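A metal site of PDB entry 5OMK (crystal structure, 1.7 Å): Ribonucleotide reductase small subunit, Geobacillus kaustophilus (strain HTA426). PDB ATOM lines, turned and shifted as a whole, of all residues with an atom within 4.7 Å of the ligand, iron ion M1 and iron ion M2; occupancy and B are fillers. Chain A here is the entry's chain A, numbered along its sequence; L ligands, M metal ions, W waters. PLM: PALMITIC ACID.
The side-chain hydroxyl (OG1) of Thr 260 sits at hydrogen-bond distance from the backbone carbonyl oxygen (O) of Val 256, 3.1 Å away.
The backbone NH (N) of Ala 185 lies within hydrogen-bond range of the backbone carbonyl oxygen (O) of Val 180, at 2.8 Å.
The backbone carbonyl oxygen (O) of Gly 78 sits at hydrogen-bond distance from the side-chain hydroxyl (OH) of Tyr 145 (2.7 Å).
OG1 of Thr 191 sits at hydrogen-bond distance from O of Ser 187 (2.8 Å).
The side-chain carboxylate (OE1) of Glu 216 sits at hydrogen-bond distance from the side-chain hydroxyl (OH) of Tyr 189, 2.5 Å away.
The side-chain hydroxyl (OH) of Tyr 145 lies within hydrogen-bond range of the backbone NH (N) of Gly 82 (3.2 Å).
Residues that only touch the ligand: Leu 75, Gly 78, Phe 79, Gly 82, Val 86, Phe 149, Val 180, Leu 184, Gly 188, Thr 191, Tyr 255, Val 256 and Leu 282.
Within 4 Å of the ligand: Leu 75, Gly 78, Phe 79, Gly 82, Glu 83, Val 86, Glu 116, His 119, Phe 149, Val 180, Glu 181, Leu 184, Gly 188, Thr 191, Glu 216, Tyr 255, Val 256 and Leu 282.
Along chain A the residues within 4 Å of the ligand span positions 75 to 282.
The nearest printed residue that does not touch the ligand is Ser 187 (4.01 Å).
Within 4 Å of iron ion M1: Glu 83, Glu 116, His 119 and Glu 216.
The nearest printed residue that does not touch iron ion M1 is Tyr 189 (4.5 Å).
Within 4 Å of iron ion M2: Glu 116, Glu 181, Glu 216 and His 219.
The nearest printed residue that does not touch iron ion M2 is Phe 112 (4.2 Å).
An oxygen (O1) of the ligand is bound to iron ion M1.
Iron ion M1 is bound by OE2 of Glu 83 (2.0 Å).
Iron ion M1 is bound by water W1.
ND1 of His 119 binds iron ion M1 (2.1 Å).
The side-chain carboxylate (OE2) of Glu 116 binds iron ion M1 (2.1 Å).
Water W2 binds iron ion M1, at 2.2 Å.
Iron ion M2 is bound by the side-chain carboxylate (OE2) of Glu 181 (2.0 Å).
Water W1 is bound to iron ion M2, at 2.0 Å.
O2 of the ligand is bound to iron ion M2 (2.0 Å).
OE1 of Glu 116 is bound to iron ion M2 (2.1 Å).
OE2 of Glu 216 binds iron ion M2 (2.2 Å).
Iron ion M2 is bound by a ring nitrogen (ND1) of His 219 (2.2 Å).
Water W2 lies within hydrogen-bond range of OE1 of Glu 83 (2.4 Å), OH of Tyr 189 (2.6 Å) and OE1 of Glu 216 (3.2 Å).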
ATOM      1  N   LEU A  75     -10.242 -24.328 -17.547  1.00  0.00           N
ATOM      2  CA  LEU A  75     -10.381 -24.460 -16.100  1.00  0.00           C
ATOM      3  C   LEU A  75      -9.158 -25.150 -15.498  1.00  0.00           C
ATOM      4  O   LEU A  75      -8.658 -24.713 -14.456  1.00  0.00           O
ATOM      5  CB  LEU A  75     -11.658 -25.214 -15.754  1.00  0.00           C
ATOM      6  CG  LEU A  75     -12.075 -25.228 -14.281  1.00  0.00           C
ATOM      7  CD1 LEU A  75     -12.264 -23.793 -13.783  1.00  0.00           C
ATOM      8  CD2 LEU A  75     -13.382 -26.070 -14.084  1.00  0.00           C
ATOM      9  N   GLY A  78      -6.299 -22.779 -15.491  1.00  0.00           N
ATOM     10  CA  GLY A  78      -6.365 -21.868 -14.361  1.00  0.00           C
ATOM     11  C   GLY A  78      -5.919 -22.531 -13.075  1.00  0.00           C
ATOM     12  O   GLY A  78      -5.190 -21.933 -12.277  1.00  0.00           O
ATOM     13  N   PHE A  79      -6.335 -23.782 -12.847  1.00  0.00           N
ATOM     14  CA  PHE A  79      -5.974 -24.439 -11.600  1.00  0.00           C
ATOM     15  C   PHE A  79      -4.489 -24.770 -11.532  1.00  0.00           C
ATOM     16  O   PHE A  79      -3.850 -24.502 -10.513  1.00  0.00           O
ATOM     17  CB  PHE A  79      -6.824 -25.677 -11.366  1.00  0.00           C
ATOM     18  CG  PHE A  79      -8.016 -25.419 -10.476  1.00  0.00           C
ATOM     19  CD1 PHE A  79      -7.856 -25.287  -9.106  1.00  0.00           C
ATOM     20  CD2 PHE A  79      -9.286 -25.308 -10.996  1.00  0.00           C
ATOM     21  CE1 PHE A  79      -8.940 -25.040  -8.279  1.00  0.00           C
ATOM     22  CE2 PHE A  79     -10.379 -25.079 -10.176  1.00  0.00           C
ATOM     23  CZ  PHE A  79     -10.214 -24.940  -8.818  1.00  0.00           C
ATOM     24  N   GLY A  82      -2.541 -21.878 -10.854  1.00  0.00           N
ATOM     25  CA  GLY A  82      -2.889 -21.405  -9.531  1.00  0.00           C
ATOM     26  C   GLY A  82      -2.179 -22.179  -8.433  1.00  0.00           C
ATOM     27  O   GLY A  82      -1.647 -21.582  -7.495  1.00  0.00           O
ATOM     28  N   GLU A  83      -2.202 -23.520  -8.531  1.00  0.00           N
ATOM     29  CA  GLU A  83      -1.556 -24.380  -7.540  1.00  0.00           C
ATOM     30  C   GLU A  83      -0.057 -24.128  -7.502  1.00  0.00           C
ATOM     31  O   GLU A  83       0.552 -24.064  -6.424  1.00  0.00           O
ATOM     32  CB  GLU A  83      -1.790 -25.855  -7.823  1.00  0.00           C
ATOM     33  CG  GLU A  83      -3.217 -26.305  -8.008  1.00  0.00           C
ATOM     34  CD  GLU A  83      -4.131 -26.098  -6.798  1.00  0.00           C
ATOM     35  OE1 GLU A  83      -5.370 -26.167  -6.982  1.00  0.00           O
ATOM     36  OE2 GLU A  83      -3.628 -25.866  -5.668  1.00  0.00           O
ATOM     37  N   VAL A  86       0.679 -20.622  -5.840  1.00  0.00           N
ATOM     38  CA  VAL A  86       0.548 -20.629  -4.369  1.00  0.00           C
ATOM     39  C   VAL A  86       1.589 -21.531  -3.691  1.00  0.00           C
ATOM     40  O   VAL A  86       2.013 -21.257  -2.563  1.00  0.00           O
ATOM     41  CB  VAL A  86      -0.887 -21.010  -3.927  1.00  0.00           C
ATOM     42  CG1 VAL A  86      -1.866 -20.002  -4.451  1.00  0.00           C
ATOM     43  CG2 VAL A  86      -1.259 -22.413  -4.366  1.00  0.00           C
ATOM     44  N   PHE A 112       0.219 -26.621   4.920  1.00  0.00           N
ATOM     45  CA  PHE A 112      -0.287 -25.781   3.835  1.00  0.00           C
ATOM     46  C   PHE A 112       0.576 -25.936   2.569  1.00  0.00           C
ATOM     47  O   PHE A 112       0.073 -26.230   1.478  1.00  0.00           O
ATOM     48  CB  PHE A 112      -0.301 -24.332   4.354  1.00  0.00           C
ATOM     49  CG  PHE A 112      -1.146 -23.344   3.575  1.00  0.00           C
ATOM     50  CD1 PHE A 112      -1.832 -22.348   4.254  1.00  0.00           C
ATOM     51  CD2 PHE A 112      -1.191 -23.342   2.203  1.00  0.00           C
ATOM     52  CE1 PHE A 112      -2.594 -21.409   3.589  1.00  0.00           C
ATOM     53  CE2 PHE A 112      -1.945 -22.387   1.526  1.00  0.00           C
ATOM     54  CZ  PHE A 112      -2.635 -21.422   2.209  1.00  0.00           C
ATOM     55  N   GLU A 116      -0.349 -27.777  -1.122  1.00  0.00           N
ATOM     56  CA  GLU A 116      -0.292 -27.147  -2.442  1.00  0.00           C
ATOM     57  C   GLU A 116       0.600 -27.917  -3.382  1.00  0.00           C
ATOM     58  O   GLU A 116       0.271 -28.034  -4.575  1.00  0.00           O
ATOM     59  CB  GLU A 116       0.164 -25.689  -2.317  1.00  0.00           C
ATOM     60  CG  GLU A 116      -0.732 -24.803  -1.453  1.00  0.00           C
ATOM     61  CD  GLU A 116      -2.175 -24.635  -1.975  1.00  0.00           C
ATOM     62  OE1 GLU A 116      -2.882 -23.774  -1.429  1.00  0.00           O
ATOM     63  OE2 GLU A 116      -2.594 -25.299  -2.948  1.00  0.00           O
ATOM     64  N   HIS A 119      -1.396 -30.550  -4.680  1.00  0.00           N
ATOM     65  CA  HIS A 119      -2.359 -30.057  -5.659  1.00  0.00           C
ATOM     66  C   HIS A 119      -1.710 -29.873  -7.023  1.00  0.00           C
ATOM     67  O   HIS A 119      -2.311 -30.220  -8.053  1.00  0.00           O
ATOM     68  CB  HIS A 119      -2.970 -28.719  -5.243  1.00  0.00           C
ATOM     69  CG  HIS A 119      -3.689 -28.759  -3.936  1.00  0.00           C
ATOM     70  ND1 HIS A 119      -4.231 -27.624  -3.343  1.00  0.00           N
ATOM     71  CD2 HIS A 119      -3.925 -29.781  -3.090  1.00  0.00           C
ATOM     72  CE1 HIS A 119      -4.803 -27.977  -2.211  1.00  0.00           C
ATOM     73  NE2 HIS A 119      -4.594 -29.266  -2.002  1.00  0.00           N
ATOM     74  N   TYR A 145      -6.414 -12.796 -15.471  1.00  0.00           N
ATOM     75  CA  TYR A 145      -5.814 -13.889 -14.739  1.00  0.00           C
ATOM     76  C   TYR A 145      -4.345 -13.590 -14.424  1.00  0.00           C
ATOM     77  O   TYR A 145      -3.879 -13.794 -13.283  1.00  0.00           O
ATOM     78  CB  TYR A 145      -5.946 -15.181 -15.546  1.00  0.00           C
ATOM     79  CG  TYR A 145      -5.394 -16.387 -14.817  1.00  0.00           C
ATOM     80  CD1 TYR A 145      -6.225 -17.236 -14.082  1.00  0.00           C
ATOM     81  CD2 TYR A 145      -4.033 -16.660 -14.874  1.00  0.00           C
ATOM     82  CE1 TYR A 145      -5.708 -18.319 -13.419  1.00  0.00           C
ATOM     83  CE2 TYR A 145      -3.503 -17.741 -14.221  1.00  0.00           C
ATOM     84  CZ  TYR A 145      -4.341 -18.559 -13.460  1.00  0.00           C
ATOM     85  OH  TYR A 145      -3.816 -19.628 -12.819  1.00  0.00           O
ATOM     86  N   PHE A 149      -2.444 -13.747 -10.780  1.00  0.00           N
ATOM     87  CA  PHE A 149      -1.534 -14.858 -10.492  1.00  0.00           C
ATOM     88  C   PHE A 149      -0.093 -14.615 -10.916  1.00  0.00           C
ATOM     89  O   PHE A 149       0.828 -15.099 -10.239  1.00  0.00           O
ATOM     90  CB  PHE A 149      -2.060 -16.117 -11.178  1.00  0.00           C
ATOM     91  CG  PHE A 149      -3.275 -16.668 -10.498  1.00  0.00           C
ATOM     92  CD1 PHE A 149      -3.130 -17.507  -9.389  1.00  0.00           C
ATOM     93  CD2 PHE A 149      -4.577 -16.357 -10.944  1.00  0.00           C
ATOM     94  CE1 PHE A 149      -4.233 -17.996  -8.733  1.00  0.00           C
ATOM     95  CE2 PHE A 149      -5.685 -16.876 -10.284  1.00  0.00           C
ATOM     96  CZ  PHE A 149      -5.504 -17.710  -9.167  1.00  0.00           C
ATOM     97  N   VAL A 180      -7.649 -15.582  -4.050  1.00  0.00           N
ATOM     98  CA  VAL A 180      -7.226 -16.722  -4.860  1.00  0.00           C
ATOM     99  C   VAL A 180      -7.889 -18.017  -4.354  1.00  0.00           C
ATOM    100  O   VAL A 180      -8.442 -18.797  -5.144  1.00  0.00           O
ATOM    101  CB  VAL A 180      -5.680 -16.811  -4.859  1.00  0.00           C
ATOM    102  CG1 VAL A 180      -5.167 -18.201  -5.214  1.00  0.00           C
ATOM    103  CG2 VAL A 180      -5.111 -15.742  -5.805  1.00  0.00           C
ATOM    104  N   GLU A 181      -7.799 -18.283  -3.058  1.00  0.00           N
ATOM    105  CA  GLU A 181      -8.381 -19.506  -2.483  1.00  0.00           C
ATOM    106  C   GLU A 181      -9.870 -19.334  -2.196  1.00  0.00           C
ATOM    107  O   GLU A 181     -10.721 -20.101  -2.673  1.00  0.00           O
ATOM    108  CB  GLU A 181      -7.636 -19.881  -1.199  1.00  0.00           C
ATOM    109  CG  GLU A 181      -6.217 -20.249  -1.447  1.00  0.00           C
ATOM    110  CD  GLU A 181      -5.470 -20.643  -0.200  1.00  0.00           C
ATOM    111  OE1 GLU A 181      -5.600 -19.944   0.820  1.00  0.00           O
ATOM    112  OE2 GLU A 181      -4.793 -21.680  -0.226  1.00  0.00           O
ATOM    113  N   LEU A 184     -11.751 -17.633  -5.840  1.00  0.00           N
ATOM    114  CA  LEU A 184     -11.541 -18.302  -7.130  1.00  0.00           C
ATOM    115  C   LEU A 184     -11.461 -19.819  -6.986  1.00  0.00           C
ATOM    116  O   LEU A 184     -12.214 -20.542  -7.655  1.00  0.00           O
ATOM    117  CB  LEU A 184     -10.308 -17.738  -7.811  1.00  0.00           C
ATOM    118  CG  LEU A 184     -10.414 -16.318  -8.366  1.00  0.00           C
ATOM    119  CD1 LEU A 184      -9.047 -15.786  -8.806  1.00  0.00           C
ATOM    120  CD2 LEU A 184     -11.387 -16.263  -9.547  1.00  0.00           C
ATOM    121  N   ALA A 185     -10.601 -20.344  -6.119  1.00  0.00           N
ATOM    122  CA  ALA A 185     -10.501 -21.802  -5.974  1.00  0.00           C
ATOM    123  C   ALA A 185     -11.846 -22.425  -5.603  1.00  0.00           C
ATOM    124  O   ALA A 185     -12.258 -23.460  -6.162  1.00  0.00           O
ATOM    125  CB  ALA A 185      -9.447 -22.182  -4.913  1.00  0.00           C
ATOM    126  N   SER A 187     -14.877 -21.342  -6.097  1.00  0.00           N
ATOM    127  CA  SER A 187     -15.803 -21.304  -7.227  1.00  0.00           C
ATOM    128  C   SER A 187     -15.373 -22.315  -8.277  1.00  0.00           C
ATOM    129  O   SER A 187     -16.204 -22.946  -8.915  1.00  0.00           O
ATOM    130  CB  SER A 187     -15.857 -19.893  -7.812  1.00  0.00           C
ATOM    131  OG  SER A 187     -16.237 -18.963  -6.814  1.00  0.00           O
ATOM    132  N   GLY A 188     -14.068 -22.507  -8.444  1.00  0.00           N
ATOM    133  CA  GLY A 188     -13.616 -23.533  -9.371  1.00  0.00           C
ATOM    134  C   GLY A 188     -14.056 -24.929  -8.981  1.00  0.00           C
ATOM    135  O   GLY A 188     -14.376 -25.742  -9.847  1.00  0.00           O
ATOM    136  N   TYR A 189     -13.986 -25.255  -7.697  1.00  0.00           N
ATOM    137  CA  TYR A 189     -14.432 -26.570  -7.246  1.00  0.00           C
ATOM    138  C   TYR A 189     -15.894 -26.749  -7.568  1.00  0.00           C
ATOM    139  O   TYR A 189     -16.323 -27.792  -8.085  1.00  0.00           O
ATOM    140  CB  TYR A 189     -14.238 -26.732  -5.737  1.00  0.00           C
ATOM    141  CG  TYR A 189     -12.807 -26.561  -5.281  1.00  0.00           C
ATOM    142  CD1 TYR A 189     -11.772 -27.027  -6.056  1.00  0.00           C
ATOM    143  CD2 TYR A 189     -12.515 -25.928  -4.056  1.00  0.00           C
ATOM    144  CE1 TYR A 189     -10.475 -26.898  -5.661  1.00  0.00           C
ATOM    145  CE2 TYR A 189     -11.225 -25.771  -3.654  1.00  0.00           C
ATOM    146  CZ  TYR A 189     -10.187 -26.254  -4.457  1.00  0.00           C
ATOM    147  OH  TYR A 189      -8.867 -26.127  -4.072  1.00  0.00           O
ATOM    148  N   THR A 191     -17.609 -25.186  -9.866  1.00  0.00           N
ATOM    149  CA  THR A 191     -17.775 -25.271 -11.323  1.00  0.00           C
ATOM    150  C   THR A 191     -17.478 -26.674 -11.829  1.00  0.00           C
ATOM    151  O   THR A 191     -18.268 -27.236 -12.610  1.00  0.00           O
ATOM    152  CB  THR A 191     -16.897 -24.222 -12.006  1.00  0.00           C
ATOM    153  OG1 THR A 191     -17.247 -22.922 -11.534  1.00  0.00           O
ATOM    154  CG2 THR A 191     -17.036 -24.234 -13.494  1.00  0.00           C
ATOM    155  N   GLU A 216      -8.614 -27.062   1.208  1.00  0.00           N
ATOM    156  CA  GLU A 216      -8.781 -25.622   1.078  1.00  0.00           C
ATOM    157  C   GLU A 216      -9.416 -25.014   2.292  1.00  0.00           C
ATOM    158  O   GLU A 216      -9.139 -23.863   2.619  1.00  0.00           O
ATOM    159  CB  GLU A 216      -9.645 -25.278  -0.148  1.00  0.00           C
ATOM    160  CG  GLU A 216      -9.382 -23.930  -0.716  1.00  0.00           C
ATOM    161  CD  GLU A 216      -8.026 -23.883  -1.362  1.00  0.00           C
ATOM    162  OE1 GLU A 216      -7.892 -24.430  -2.495  1.00  0.00           O
ATOM    163  OE2 GLU A 216      -7.081 -23.397  -0.688  1.00  0.00           O
ATOM    164  N   HIS A 219      -6.720 -23.873   4.524  1.00  0.00           N
ATOM    165  CA  HIS A 219      -6.019 -22.723   3.955  1.00  0.00           C
ATOM    166  C   HIS A 219      -6.799 -21.438   4.194  1.00  0.00           C
ATOM    167  O   HIS A 219      -6.248 -20.408   4.607  1.00  0.00           O
ATOM    168  CB  HIS A 219      -5.807 -22.951   2.433  1.00  0.00           C
ATOM    169  CG  HIS A 219      -5.065 -24.203   2.130  1.00  0.00           C
ATOM    170  ND1 HIS A 219      -4.758 -24.604   0.840  1.00  0.00           N
ATOM    171  CD2 HIS A 219      -4.611 -25.182   2.954  1.00  0.00           C
ATOM    172  CE1 HIS A 219      -4.131 -25.773   0.895  1.00  0.00           C
ATOM    173  NE2 HIS A 219      -4.023 -26.134   2.162  1.00  0.00           N
ATOM    174  N   TYR A 255     -11.759 -12.390 -15.144  1.00  0.00           N
ATOM    175  CA  TYR A 255     -11.371 -13.739 -15.510  1.00  0.00           C
ATOM    176  C   TYR A 255     -12.605 -14.634 -15.621  1.00  0.00           C
ATOM    177  O   TYR A 255     -12.712 -15.455 -16.545  1.00  0.00           O
ATOM    178  CB  TYR A 255     -10.389 -14.279 -14.474  1.00  0.00           C
ATOM    179  CG  TYR A 255      -9.997 -15.720 -14.686  1.00  0.00           C
ATOM    180  CD1 TYR A 255      -9.419 -16.135 -15.875  1.00  0.00           C
ATOM    181  CD2 TYR A 255     -10.185 -16.662 -13.681  1.00  0.00           C
ATOM    182  CE1 TYR A 255      -9.047 -17.482 -16.068  1.00  0.00           C
ATOM    183  CE2 TYR A 255      -9.804 -18.013 -13.865  1.00  0.00           C
ATOM    184  CZ  TYR A 255      -9.234 -18.399 -15.046  1.00  0.00           C
ATOM    185  OH  TYR A 255      -8.857 -19.719 -15.264  1.00  0.00           O
ATOM    186  N   VAL A 256     -13.531 -14.510 -14.682  1.00  0.00           N
ATOM    187  CA  VAL A 256     -14.756 -15.318 -14.725  1.00  0.00           C
ATOM    188  C   VAL A 256     -15.504 -15.058 -16.024  1.00  0.00           C
ATOM    189  O   VAL A 256     -15.945 -15.983 -16.698  1.00  0.00           O
ATOM    190  CB  VAL A 256     -15.622 -15.040 -13.487  1.00  0.00           C
ATOM    191  CG1 VAL A 256     -17.008 -15.667 -13.639  1.00  0.00           C
ATOM    192  CG2 VAL A 256     -14.977 -15.607 -12.232  1.00  0.00           C
ATOM    193  N   LEU A 259     -13.809 -16.872 -18.923  1.00  0.00           N
ATOM    194  CA  LEU A 259     -14.083 -18.301 -18.979  1.00  0.00           C
ATOM    195  C   LEU A 259     -15.520 -18.569 -19.421  1.00  0.00           C
ATOM    196  O   LEU A 259     -15.775 -19.551 -20.125  1.00  0.00           O
ATOM    197  CB  LEU A 259     -13.866 -18.945 -17.627  1.00  0.00           C
ATOM    198  CG  LEU A 259     -12.434 -18.985 -17.122  1.00  0.00           C
ATOM    199  CD1 LEU A 259     -12.502 -19.610 -15.741  1.00  0.00           C
ATOM    200  CD2 LEU A 259     -11.547 -19.786 -18.058  1.00  0.00           C
ATOM    201  N   THR A 260     -16.458 -17.746 -18.952  1.00  0.00           N
ATOM    202  CA  THR A 260     -17.842 -17.890 -19.372  1.00  0.00           C
ATOM    203  C   THR A 260     -17.977 -17.680 -20.880  1.00  0.00           C
ATOM    204  O   THR A 260     -18.647 -18.461 -21.565  1.00  0.00           O
ATOM    205  CB  THR A 260     -18.704 -16.882 -18.628  1.00  0.00           C
ATOM    206  OG1 THR A 260     -18.730 -17.232 -17.245  1.00  0.00           O
ATOM    207  CG2 THR A 260     -20.149 -16.891 -19.196  1.00  0.00           C
ATOM    208  N   TYR A 279     -24.300 -20.617 -16.632  1.00  0.00           N
ATOM    209  CA  TYR A 279     -23.208 -19.682 -16.379  1.00  0.00           C
ATOM    210  C   TYR A 279     -23.653 -18.518 -15.501  1.00  0.00           C
ATOM    211  O   TYR A 279     -22.886 -18.039 -14.668  1.00  0.00           O
ATOM    212  CB  TYR A 279     -22.616 -19.175 -17.694  1.00  0.00           C
ATOM    213  CG  TYR A 279     -21.871 -20.253 -18.404  1.00  0.00           C
ATOM    214  CD1 TYR A 279     -20.683 -20.735 -17.900  1.00  0.00           C
ATOM    215  CD2 TYR A 279     -22.370 -20.824 -19.569  1.00  0.00           C
ATOM    216  CE1 TYR A 279     -19.996 -21.746 -18.526  1.00  0.00           C
ATOM    217  CE2 TYR A 279     -21.684 -21.838 -20.215  1.00  0.00           C
ATOM    218  CZ  TYR A 279     -20.494 -22.294 -19.684  1.00  0.00           C
ATOM    219  OH  TYR A 279     -19.807 -23.304 -20.300  1.00  0.00           O
ATOM    220  N   LEU A 282     -23.149 -19.842 -12.067  1.00  0.00           N
ATOM    221  CA  LEU A 282     -21.745 -19.877 -11.693  1.00  0.00           C
ATOM    222  C   LEU A 282     -21.256 -18.473 -11.369  1.00  0.00           C
ATOM    223  O   LEU A 282     -20.557 -18.264 -10.375  1.00  0.00           O
ATOM    224  CB  LEU A 282     -20.914 -20.494 -12.813  1.00  0.00           C
ATOM    225  CG  LEU A 282     -21.186 -21.959 -13.157  1.00  0.00           C
ATOM    226  CD1 LEU A 282     -20.367 -22.389 -14.363  1.00  0.00           C
ATOM    227  CD2 LEU A 282     -20.941 -22.882 -11.959  1.00  0.00           C
ATOM    228  N   VAL A 286     -19.639 -17.014  -7.633  1.00  0.00           N
ATOM    229  CA  VAL A 286     -18.414 -16.238  -7.434  1.00  0.00           C
ATOM    230  C   VAL A 286     -18.703 -14.995  -6.613  1.00  0.00           C
ATOM    231  O   VAL A 286     -17.990 -14.696  -5.652  1.00  0.00           O
ATOM    232  CB  VAL A 286     -17.778 -15.865  -8.794  1.00  0.00           C
ATOM    233  CG1 VAL A 286     -16.571 -14.953  -8.592  1.00  0.00           C
ATOM    234  CG2 VAL A 286     -17.360 -17.094  -9.530  1.00  0.00           C
HETATM  235  C1  PLM L   1      -4.949 -22.932  -4.190  1.00  0.00           C
HETATM  236  O1  PLM L   1      -4.595 -24.012  -4.702  1.00  0.00           O
HETATM  237  O2  PLM L   1      -4.941 -22.602  -2.942  1.00  0.00           O
HETATM  238  C2  PLM L   1      -5.438 -21.838  -5.199  1.00  0.00           C
HETATM  239  C3  PLM L   1      -5.763 -22.305  -6.567  1.00  0.00           C
HETATM  240  C4  PLM L   1      -6.316 -21.221  -7.492  1.00  0.00           C
HETATM  241  C5  PLM L   1      -7.076 -21.753  -8.712  1.00  0.00           C
HETATM  242  C6  PLM L   1      -7.436 -20.692  -9.712  1.00  0.00           C
HETATM  243  C7  PLM L   1      -8.260 -21.153 -10.909  1.00  0.00           C
HETATM  244  C8  PLM L   1      -9.628 -21.474 -10.518  1.00  0.00           C
HETATM  245  C9  PLM L   1     -10.624 -21.396 -11.631  1.00  0.00           C
HETATM  246  CA  PLM L   1     -11.694 -20.338 -11.340  1.00  0.00           C
HETATM  247  CB  PLM L   1     -13.011 -20.707 -11.874  1.00  0.00           C
HETATM  248  CC  PLM L   1     -14.118 -19.752 -11.425  1.00  0.00           C
HETATM  249  CD  PLM L   1     -15.482 -20.189 -11.968  1.00  0.00           C
HETATM  250  CE  PLM L   1     -15.924 -19.497 -13.268  1.00  0.00           C
HETATM  251  CF  PLM L   1     -17.138 -20.151 -13.959  1.00  0.00           C
HETATM  252  CG  PLM L   1     -16.948 -20.423 -15.474  1.00  0.00           C
HETATM  253 FE    FE M   1      -4.437 -25.636  -3.819  1.00  0.00          FE
HETATM  254 FE    FE M   2      -4.955 -23.505  -1.111  1.00  0.00          FE
HETATM  255  O   HOH W   1      -5.452 -25.224  -2.088  1.00  0.00           O
HETATM  256  O   HOH W   2      -6.377 -26.140  -4.765  1.00  0.00           O
